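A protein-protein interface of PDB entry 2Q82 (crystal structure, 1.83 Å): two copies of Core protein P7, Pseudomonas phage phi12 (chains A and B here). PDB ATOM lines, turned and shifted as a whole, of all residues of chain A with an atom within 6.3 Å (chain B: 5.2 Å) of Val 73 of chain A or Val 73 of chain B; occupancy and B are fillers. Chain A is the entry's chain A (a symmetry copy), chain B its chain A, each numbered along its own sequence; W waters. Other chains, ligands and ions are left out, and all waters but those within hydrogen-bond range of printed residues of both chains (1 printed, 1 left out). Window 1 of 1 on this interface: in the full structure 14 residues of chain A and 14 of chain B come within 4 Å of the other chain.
The guanidinium group (NH1) of Arg 77 of chain A lies within salt-bridge range of the side-chain carboxylate (OD1) of Asp 69 of chain B (2.8 Å). NH1 of Arg 77 of chain B is in salt-bridge range of OD1 of Asp 69 of chain A (2.8 Å).
CB of Ala 80 of chain B touches C of Asp 69 of chain A, 3.8 Å away. Ala 80 of chain B touches Leu 70 of chain A. NH2 of Arg 77 of chain B touches CD1 of Tyr 72 of chain A, 3.4 Å away. Val 73 of chain A touches Val 73 of chain B (CG2 to CG1, 3.9 Å). CB of Ala 80 of chain B touches CG2 of Val 73 of chain A, 3.96 Å away. Arg 77 of chain A touches Tyr 72 of chain B. Asp 69 of chain B touches Leu 79 of chain A. Ala 80 of chain A touches Asp 69 of chain B. Leu 70 of chain B touches Ala 80 of chain A (CA to CB, 3.7 Å). Ala 80 of chain A touches Val 73 of chain B (CB to CG2, 3.96 Å).
Gln 68 of chain A touches none of the printed residues of chain B. Of the printed residues of chain B, Leu 79 of chain A touches Asp 69 (3.5 Å). Glu 103 of chain A touches none of the printed residues of chain B. Of the printed residues of chain A, Asp 69 of chain B touches Arg 77 (2.8 Å), Leu 79 (3.5 Å) and Ala 80 (3.8 Å). Printed residues of chain A within 4 Å of Tyr 72 of chain B: Arg 77 (3.4 Å). Val 73 of chain B touches just these residues of chain A: Val 73 (3.9 Å) and Ala 80 (3.96 Å). Printed residues of chain A within 4 Å of Arg 77 of chain B: Asp 69 (2.8 Å) and Tyr 72 (3.4 Å). Of the printed residues of chain A, Ala 80 of chain B touches Asp 69, Leu 70 and Val 73.
Along chain B the printed residues that touch a printed residue of chain A span positions 69 to 80. Printed residues of chain A that touch a printed residue of chain B: Asp 69, Leu 70, Tyr 72, Val 73, Arg 77, Leu 79 and Ala 80. Among the printed residues, 12 pairs touch across the chains.
Leu 70 of chain A touches Ala 80 of chain B, and with the chains exchanged Ala 80 of chain A touches Leu 70 of chain B. Tyr 72 of chain A touches Arg 77 of chain B, and with the chains exchanged Arg 77 of chain A touches Tyr 72 of chain B. Val 73 of chain B touches its own counterpart, Val 73 of chain A. Val 73 of chain A touches Ala 80 of chain B, and with the chains exchanged Ala 80 of chain A touches Val 73 of chain B. Positions printed for both chains: 69, 70, 71, 72, 73, 74, 75, 76, 77, 78, 80 and 81.
Water W1 lies within hydrogen-bond range of N of Leu 79 of chain A (2.8 Å) and OD2 of Asp 69 of chain B (3.0 Å).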
ATOM      1  N   GLN A  68      -7.324  19.657 -32.620  1.00  0.00           N
ATOM      2  CA  GLN A  68      -7.134  19.949 -31.218  1.00  0.00           C
ATOM      3  C   GLN A  68      -8.001  19.069 -30.320  1.00  0.00           C
ATOM      4  O   GLN A  68      -7.501  18.434 -29.393  1.00  0.00           O
ATOM      5  CB  GLN A  68      -7.462  21.421 -30.984  1.00  0.00           C
ATOM      6  CG  GLN A  68      -7.463  21.846 -29.546  1.00  0.00           C
ATOM      7  CD  GLN A  68      -7.932  23.277 -29.360  1.00  0.00           C
ATOM      8  OE1 GLN A  68      -8.170  23.715 -28.238  1.00  0.00           O
ATOM      9  NE2 GLN A  68      -8.065  24.014 -30.461  1.00  0.00           N
ATOM     10  N   ASP A  69      -9.297  19.001 -30.602  1.00  0.00           N
ATOM     11  CA  ASP A  69     -10.164  18.213 -29.744  1.00  0.00           C
ATOM     12  C   ASP A  69      -9.965  16.708 -29.825  1.00  0.00           C
ATOM     13  O   ASP A  69     -10.026  16.010 -28.816  1.00  0.00           O
ATOM     14  CB  ASP A  69     -11.628  18.554 -29.996  1.00  0.00           C
ATOM     15  CG  ASP A  69     -11.957  19.984 -29.626  1.00  0.00           C
ATOM     16  OD1 ASP A  69     -11.400  20.481 -28.626  1.00  0.00           O
ATOM     17  OD2 ASP A  69     -12.772  20.602 -30.333  1.00  0.00           O
ATOM     18  N   LEU A  70      -9.730  16.203 -31.023  1.00  0.00           N
ATOM     19  CA  LEU A  70      -9.542  14.784 -31.167  1.00  0.00           C
ATOM     20  C   LEU A  70      -8.231  14.361 -30.496  1.00  0.00           C
ATOM     21  O   LEU A  70      -8.162  13.314 -29.871  1.00  0.00           O
ATOM     22  CB  LEU A  70      -9.520  14.410 -32.636  1.00  0.00           C
ATOM     23  CG  LEU A  70      -9.278  12.945 -32.919  1.00  0.00           C
ATOM     24  CD1 LEU A  70     -10.365  12.079 -32.294  1.00  0.00           C
ATOM     25  CD2 LEU A  70      -9.256  12.765 -34.408  1.00  0.00           C
ATOM     26  N   ALA A  71      -7.200  15.186 -30.642  1.00  0.00           N
ATOM     27  CA  ALA A  71      -5.908  14.890 -30.050  1.00  0.00           C
ATOM     28  C   ALA A  71      -6.073  14.818 -28.540  1.00  0.00           C
ATOM     29  O   ALA A  71      -5.504  13.966 -27.874  1.00  0.00           O
ATOM     30  CB  ALA A  71      -4.906  15.969 -30.402  1.00  0.00           C
ATOM     31  N   TYR A  72      -6.851  15.746 -28.008  1.00  0.00           N
ATOM     32  CA  TYR A  72      -7.065  15.771 -26.592  1.00  0.00           C
ATOM     33  C   TYR A  72      -7.698  14.453 -26.131  1.00  0.00           C
ATOM     34  O   TYR A  72      -7.276  13.854 -25.140  1.00  0.00           O
ATOM     35  CB  TYR A  72      -7.973  16.922 -26.232  1.00  0.00           C
ATOM     36  CG  TYR A  72      -8.255  16.912 -24.780  1.00  0.00           C
ATOM     37  CD1 TYR A  72      -7.358  17.474 -23.882  1.00  0.00           C
ATOM     38  CD2 TYR A  72      -9.381  16.268 -24.292  1.00  0.00           C
ATOM     39  CE1 TYR A  72      -7.580  17.397 -22.531  1.00  0.00           C
ATOM     40  CE2 TYR A  72      -9.615  16.181 -22.946  1.00  0.00           C
ATOM     41  CZ  TYR A  72      -8.711  16.747 -22.068  1.00  0.00           C
ATOM     42  OH  TYR A  72      -8.950  16.692 -20.728  1.00  0.00           O
ATOM     43  N   VAL A  73      -8.710  14.011 -26.862  1.00  0.00           N
ATOM     44  CA  VAL A  73      -9.381  12.773 -26.507  1.00  0.00           C
ATOM     45  C   VAL A  73      -8.416  11.578 -26.505  1.00  0.00           C
ATOM     46  O   VAL A  73      -8.375  10.804 -25.554  1.00  0.00           O
ATOM     47  CB  VAL A  73     -10.534  12.503 -27.455  1.00  0.00           C
ATOM     48  CG1 VAL A  73     -11.112  11.138 -27.192  1.00  0.00           C
ATOM     49  CG2 VAL A  73     -11.596  13.573 -27.265  1.00  0.00           C
ATOM     50  N   PHE A  74      -7.645  11.434 -27.578  1.00  0.00           N
ATOM     51  CA  PHE A  74      -6.683  10.339 -27.661  1.00  0.00           C
ATOM     52  C   PHE A  74      -5.697  10.389 -26.495  1.00  0.00           C
ATOM     53  O   PHE A  74      -5.314   9.359 -25.936  1.00  0.00           O
ATOM     54  CB  PHE A  74      -5.865  10.426 -28.947  1.00  0.00           C
ATOM     55  CG  PHE A  74      -6.630  10.098 -30.198  1.00  0.00           C
ATOM     56  CD1 PHE A  74      -7.826   9.385 -30.155  1.00  0.00           C
ATOM     57  CD2 PHE A  74      -6.089  10.425 -31.438  1.00  0.00           C
ATOM     58  CE1 PHE A  74      -8.480   9.016 -31.339  1.00  0.00           C
ATOM     59  CE2 PHE A  74      -6.725  10.065 -32.618  1.00  0.00           C
ATOM     60  CZ  PHE A  74      -7.924   9.346 -32.572  1.00  0.00           C
ATOM     61  N   GLY A  75      -5.278  11.598 -26.141  1.00  0.00           N
ATOM     62  CA  GLY A  75      -4.292  11.745 -25.093  1.00  0.00           C
ATOM     63  C   GLY A  75      -4.773  11.719 -23.662  1.00  0.00           C
ATOM     64  O   GLY A  75      -4.038  11.302 -22.761  1.00  0.00           O
ATOM     65  N   ALA A  76      -6.010  12.143 -23.450  1.00  0.00           N
ATOM     66  CA  ALA A  76      -6.564  12.213 -22.113  1.00  0.00           C
ATOM     67  C   ALA A  76      -7.729  11.281 -21.833  1.00  0.00           C
ATOM     68  O   ALA A  76      -8.007  10.989 -20.679  1.00  0.00           O
ATOM     69  CB  ALA A  76      -6.970  13.647 -21.805  1.00  0.00           C
ATOM     70  N   ARG A  77      -8.429  10.825 -22.863  1.00  0.00           N
ATOM     71  CA  ARG A  77      -9.558   9.935 -22.631  1.00  0.00           C
ATOM     72  C   ARG A  77      -9.463   8.713 -23.528  1.00  0.00           C
ATOM     73  O   ARG A  77     -10.374   8.377 -24.283  1.00  0.00           O
ATOM     74  CB  ARG A  77     -10.878  10.672 -22.870  1.00  0.00           C
ATOM     75  CG  ARG A  77     -11.102  11.870 -21.938  1.00  0.00           C
ATOM     76  CD  ARG A  77     -11.568  11.472 -20.535  1.00  0.00           C
ATOM     77  NE  ARG A  77     -11.803  12.667 -19.722  1.00  0.00           N
ATOM     78  CZ  ARG A  77     -12.512  12.699 -18.600  1.00  0.00           C
ATOM     79  NH1 ARG A  77     -13.082  11.601 -18.128  1.00  0.00           N
ATOM     80  NH2 ARG A  77     -12.651  13.841 -17.940  1.00  0.00           N
ATOM     81  N   PRO A  78      -8.336   8.001 -23.437  1.00  0.00           N
ATOM     82  CA  PRO A  78      -8.080   6.809 -24.231  1.00  0.00           C
ATOM     83  C   PRO A  78      -9.169   5.776 -24.207  1.00  0.00           C
ATOM     84  O   PRO A  78      -9.461   5.172 -25.222  1.00  0.00           O
ATOM     85  CB  PRO A  78      -6.781   6.270 -23.661  1.00  0.00           C
ATOM     86  CG  PRO A  78      -6.707   6.789 -22.359  1.00  0.00           C
ATOM     87  CD  PRO A  78      -7.333   8.135 -22.369  1.00  0.00           C
ATOM     88  N   LEU A  79      -9.778   5.536 -23.054  1.00  0.00           N
ATOM     89  CA  LEU A  79     -10.813   4.524 -22.962  1.00  0.00           C
ATOM     90  C   LEU A  79     -12.110   4.835 -23.710  1.00  0.00           C
ATOM     91  O   LEU A  79     -12.956   3.963 -23.854  1.00  0.00           O
ATOM     92  CB  LEU A  79     -11.123   4.275 -21.493  1.00  0.00           C
ATOM     93  CG  LEU A  79      -9.913   3.944 -20.620  1.00  0.00           C
ATOM     94  CD1 LEU A  79     -10.377   3.807 -19.204  1.00  0.00           C
ATOM     95  CD2 LEU A  79      -9.232   2.671 -21.079  1.00  0.00           C
ATOM     96  N   ALA A  80     -12.271   6.067 -24.184  1.00  0.00           N
ATOM     97  CA  ALA A  80     -13.490   6.438 -24.891  1.00  0.00           C
ATOM     98  C   ALA A  80     -13.392   6.122 -26.361  1.00  0.00           C
ATOM     99  O   ALA A  80     -14.380   6.157 -27.090  1.00  0.00           O
ATOM    100  CB  ALA A  80     -13.756   7.916 -24.722  1.00  0.00           C
ATOM    101  N   VAL A  81     -12.175   5.832 -26.796  1.00  0.00           N
ATOM    102  CA  VAL A  81     -11.931   5.573 -28.194  1.00  0.00           C
ATOM    103  C   VAL A  81     -12.434   4.216 -28.664  1.00  0.00           C
ATOM    104  O   VAL A  81     -13.226   4.137 -29.595  1.00  0.00           O
ATOM    105  CB  VAL A  81     -10.435   5.697 -28.479  1.00  0.00           C
ATOM    106  CG1 VAL A  81     -10.134   5.419 -29.884  1.00  0.00           C
ATOM    107  CG2 VAL A  81      -9.958   7.089 -28.103  1.00  0.00           C
ATOM    108  N   GLU A 103      -0.944  17.458 -26.548  1.00  0.00           N
ATOM    109  CA  GLU A 103      -2.172  16.751 -26.259  1.00  0.00           C
ATOM    110  C   GLU A 103      -1.955  15.256 -26.139  1.00  0.00           C
ATOM    111  O   GLU A 103      -2.599  14.597 -25.337  1.00  0.00           O
ATOM    112  CB  GLU A 103      -3.172  17.015 -27.361  1.00  0.00           C
ATOM    113  CG  GLU A 103      -3.490  18.461 -27.488  1.00  0.00           C
ATOM    114  CD  GLU A 103      -4.628  18.847 -26.604  1.00  0.00           C
ATOM    115  OE1 GLU A 103      -4.576  18.549 -25.392  1.00  0.00           O
ATOM    116  OE2 GLU A 103      -5.583  19.443 -27.134  1.00  0.00           O
ATOM    117  N   ASP B  69     -15.831   8.123 -19.476  1.00  0.00           N
ATOM    118  CA  ASP B  69     -14.997   8.834 -20.429  1.00  0.00           C
ATOM    119  C   ASP B  69     -15.678   9.209 -21.735  1.00  0.00           C
ATOM    120  O   ASP B  69     -15.452  10.291 -22.273  1.00  0.00           O
ATOM    121  CB  ASP B  69     -13.721   8.052 -20.719  1.00  0.00           C
ATOM    122  CG  ASP B  69     -12.838   7.918 -19.496  1.00  0.00           C
ATOM    123  OD1 ASP B  69     -12.773   8.880 -18.705  1.00  0.00           O
ATOM    124  OD2 ASP B  69     -12.213   6.855 -19.336  1.00  0.00           O
ATOM    125  N   LEU B  70     -16.507   8.321 -22.250  1.00  0.00           N
ATOM    126  CA  LEU B  70     -17.178   8.613 -23.490  1.00  0.00           C
ATOM    127  C   LEU B  70     -18.184   9.750 -23.283  1.00  0.00           C
ATOM    128  O   LEU B  70     -18.331  10.611 -24.136  1.00  0.00           O
ATOM    129  CB  LEU B  70     -17.887   7.374 -24.001  1.00  0.00           C
ATOM    130  CG  LEU B  70     -18.672   7.569 -25.278  1.00  0.00           C
ATOM    131  CD1 LEU B  70     -17.763   8.018 -26.416  1.00  0.00           C
ATOM    132  CD2 LEU B  70     -19.328   6.263 -25.614  1.00  0.00           C
ATOM    133  N   ALA B  71     -18.869   9.732 -22.146  1.00  0.00           N
ATOM    134  CA  ALA B  71     -19.850  10.759 -21.840  1.00  0.00           C
ATOM    135  C   ALA B  71     -19.142  12.103 -21.787  1.00  0.00           C
ATOM    136  O   ALA B  71     -19.644  13.110 -22.263  1.00  0.00           O
ATOM    137  CB  ALA B  71     -20.511  10.478 -20.508  1.00  0.00           C
ATOM    138  N   TYR B  72     -17.967  12.104 -21.178  1.00  0.00           N
ATOM    139  CA  TYR B  72     -17.222  13.322 -21.068  1.00  0.00           C
ATOM    140  C   TYR B  72     -16.913  13.880 -22.461  1.00  0.00           C
ATOM    141  O   TYR B  72     -17.082  15.073 -22.723  1.00  0.00           O
ATOM    142  CB  TYR B  72     -15.932  13.067 -20.327  1.00  0.00           C
ATOM    143  CG  TYR B  72     -15.125  14.305 -20.270  1.00  0.00           C
ATOM    144  CD1 TYR B  72     -15.372  15.265 -19.299  1.00  0.00           C
ATOM    145  CD2 TYR B  72     -14.165  14.559 -21.238  1.00  0.00           C
ATOM    146  CE1 TYR B  72     -14.679  16.448 -19.291  1.00  0.00           C
ATOM    147  CE2 TYR B  72     -13.466  15.736 -21.245  1.00  0.00           C
ATOM    148  CZ  TYR B  72     -13.726  16.679 -20.269  1.00  0.00           C
ATOM    149  OH  TYR B  72     -13.015  17.841 -20.250  1.00  0.00           O
ATOM    150  N   VAL B  73     -16.464  13.005 -23.348  1.00  0.00           N
ATOM    151  CA  VAL B  73     -16.138  13.435 -24.697  1.00  0.00           C
ATOM    152  C   VAL B  73     -17.350  14.050 -25.411  1.00  0.00           C
ATOM    153  O   VAL B  73     -17.261  15.129 -25.986  1.00  0.00           O
ATOM    154  CB  VAL B  73     -15.596  12.273 -25.507  1.00  0.00           C
ATOM    155  CG1 VAL B  73     -15.427  12.680 -26.947  1.00  0.00           C
ATOM    156  CG2 VAL B  73     -14.265  11.834 -24.922  1.00  0.00           C
ATOM    157  N   PHE B  74     -18.481  13.352 -25.372  1.00  0.00           N
ATOM    158  CA  PHE B  74     -19.693  13.863 -26.007  1.00  0.00           C
ATOM    159  C   PHE B  74     -20.075  15.227 -25.436  1.00  0.00           C
ATOM    160  O   PHE B  74     -20.515  16.123 -26.159  1.00  0.00           O
ATOM    161  CB  PHE B  74     -20.874  12.925 -25.765  1.00  0.00           C
ATOM    162  CG  PHE B  74     -20.804  11.625 -26.515  1.00  0.00           C
ATOM    163  CD1 PHE B  74     -19.979  11.468 -27.626  1.00  0.00           C
ATOM    164  CD2 PHE B  74     -21.651  10.580 -26.156  1.00  0.00           C
ATOM    165  CE1 PHE B  74     -19.992  10.274 -28.362  1.00  0.00           C
ATOM    166  CE2 PHE B  74     -21.675   9.393 -26.875  1.00  0.00           C
ATOM    167  CZ  PHE B  74     -20.848   9.240 -27.994  1.00  0.00           C
ATOM    168  N   GLY B  75     -19.916  15.373 -24.126  1.00  0.00           N
ATOM    169  CA  GLY B  75     -20.313  16.604 -23.481  1.00  0.00           C
ATOM    170  C   GLY B  75     -19.348  17.764 -23.517  1.00  0.00           C
ATOM    171  O   GLY B  75     -19.764  18.927 -23.502  1.00  0.00           O
ATOM    172  N   ALA B  76     -18.061  17.457 -23.587  1.00  0.00           N
ATOM    173  CA  ALA B  76     -17.038  18.484 -23.577  1.00  0.00           C
ATOM    174  C   ALA B  76     -16.218  18.609 -24.848  1.00  0.00           C
ATOM    175  O   ALA B  76     -15.620  19.649 -25.082  1.00  0.00           O
ATOM    176  CB  ALA B  76     -16.112  18.267 -22.389  1.00  0.00           C
ATOM    177  N   ARG B  77     -16.158  17.563 -25.662  1.00  0.00           N
ATOM    178  CA  ARG B  77     -15.375  17.646 -26.886  1.00  0.00           C
ATOM    179  C   ARG B  77     -16.195  17.171 -28.073  1.00  0.00           C
ATOM    180  O   ARG B  77     -15.808  16.279 -28.827  1.00  0.00           O
ATOM    181  CB  ARG B  77     -14.092  16.819 -26.757  1.00  0.00           C
ATOM    182  CG  ARG B  77     -13.156  17.291 -25.638  1.00  0.00           C
ATOM    183  CD  ARG B  77     -12.333  18.526 -26.012  1.00  0.00           C
ATOM    184  NE  ARG B  77     -11.433  18.887 -24.914  1.00  0.00           N
ATOM    185  CZ  ARG B  77     -10.372  19.679 -25.025  1.00  0.00           C
ATOM    186  NH1 ARG B  77     -10.044  20.211 -26.193  1.00  0.00           N
ATOM    187  NH2 ARG B  77      -9.633  19.943 -23.957  1.00  0.00           N
ATOM    188  N   PRO B  78     -17.359  17.794 -28.273  1.00  0.00           N
ATOM    189  CA  PRO B  78     -18.268  17.456 -29.358  1.00  0.00           C
ATOM    190  C   PRO B  78     -17.645  17.399 -30.723  1.00  0.00           C
ATOM    191  O   PRO B  78     -17.980  16.535 -31.511  1.00  0.00           O
ATOM    192  CB  PRO B  78     -19.340  18.528 -29.275  1.00  0.00           C
ATOM    193  CG  PRO B  78     -18.732  19.607 -28.614  1.00  0.00           C
ATOM    194  CD  PRO B  78     -17.767  19.053 -27.630  1.00  0.00           C
ATOM    195  N   ALA B  80     -14.863  16.361 -31.663  1.00  0.00           N
ATOM    196  CA  ALA B  80     -13.966  15.233 -31.885  1.00  0.00           C
ATOM    197  C   ALA B  80     -14.724  14.003 -32.314  1.00  0.00           C
ATOM    198  O   ALA B  80     -14.143  13.015 -32.756  1.00  0.00           O
ATOM    199  CB  ALA B  80     -13.201  14.923 -30.619  1.00  0.00           C
ATOM    200  N   VAL B  81     -16.037  14.066 -32.158  1.00  0.00           N
ATOM    201  CA  VAL B  81     -16.875  12.934 -32.468  1.00  0.00           C
ATOM    202  C   VAL B  81     -17.055  12.694 -33.960  1.00  0.00           C
ATOM    203  O   VAL B  81     -16.757  11.614 -34.454  1.00  0.00           O
ATOM    204  CB  VAL B  81     -18.241  13.117 -31.807  1.00  0.00           C
ATOM    205  CG1 VAL B  81     -19.137  12.001 -32.113  1.00  0.00           C
ATOM    206  CG2 VAL B  81     -18.065  13.254 -30.304  1.00  0.00           C
HETATM  207  O   HOH W   1      -9.628   7.101 -20.754  1.00  0.00           O
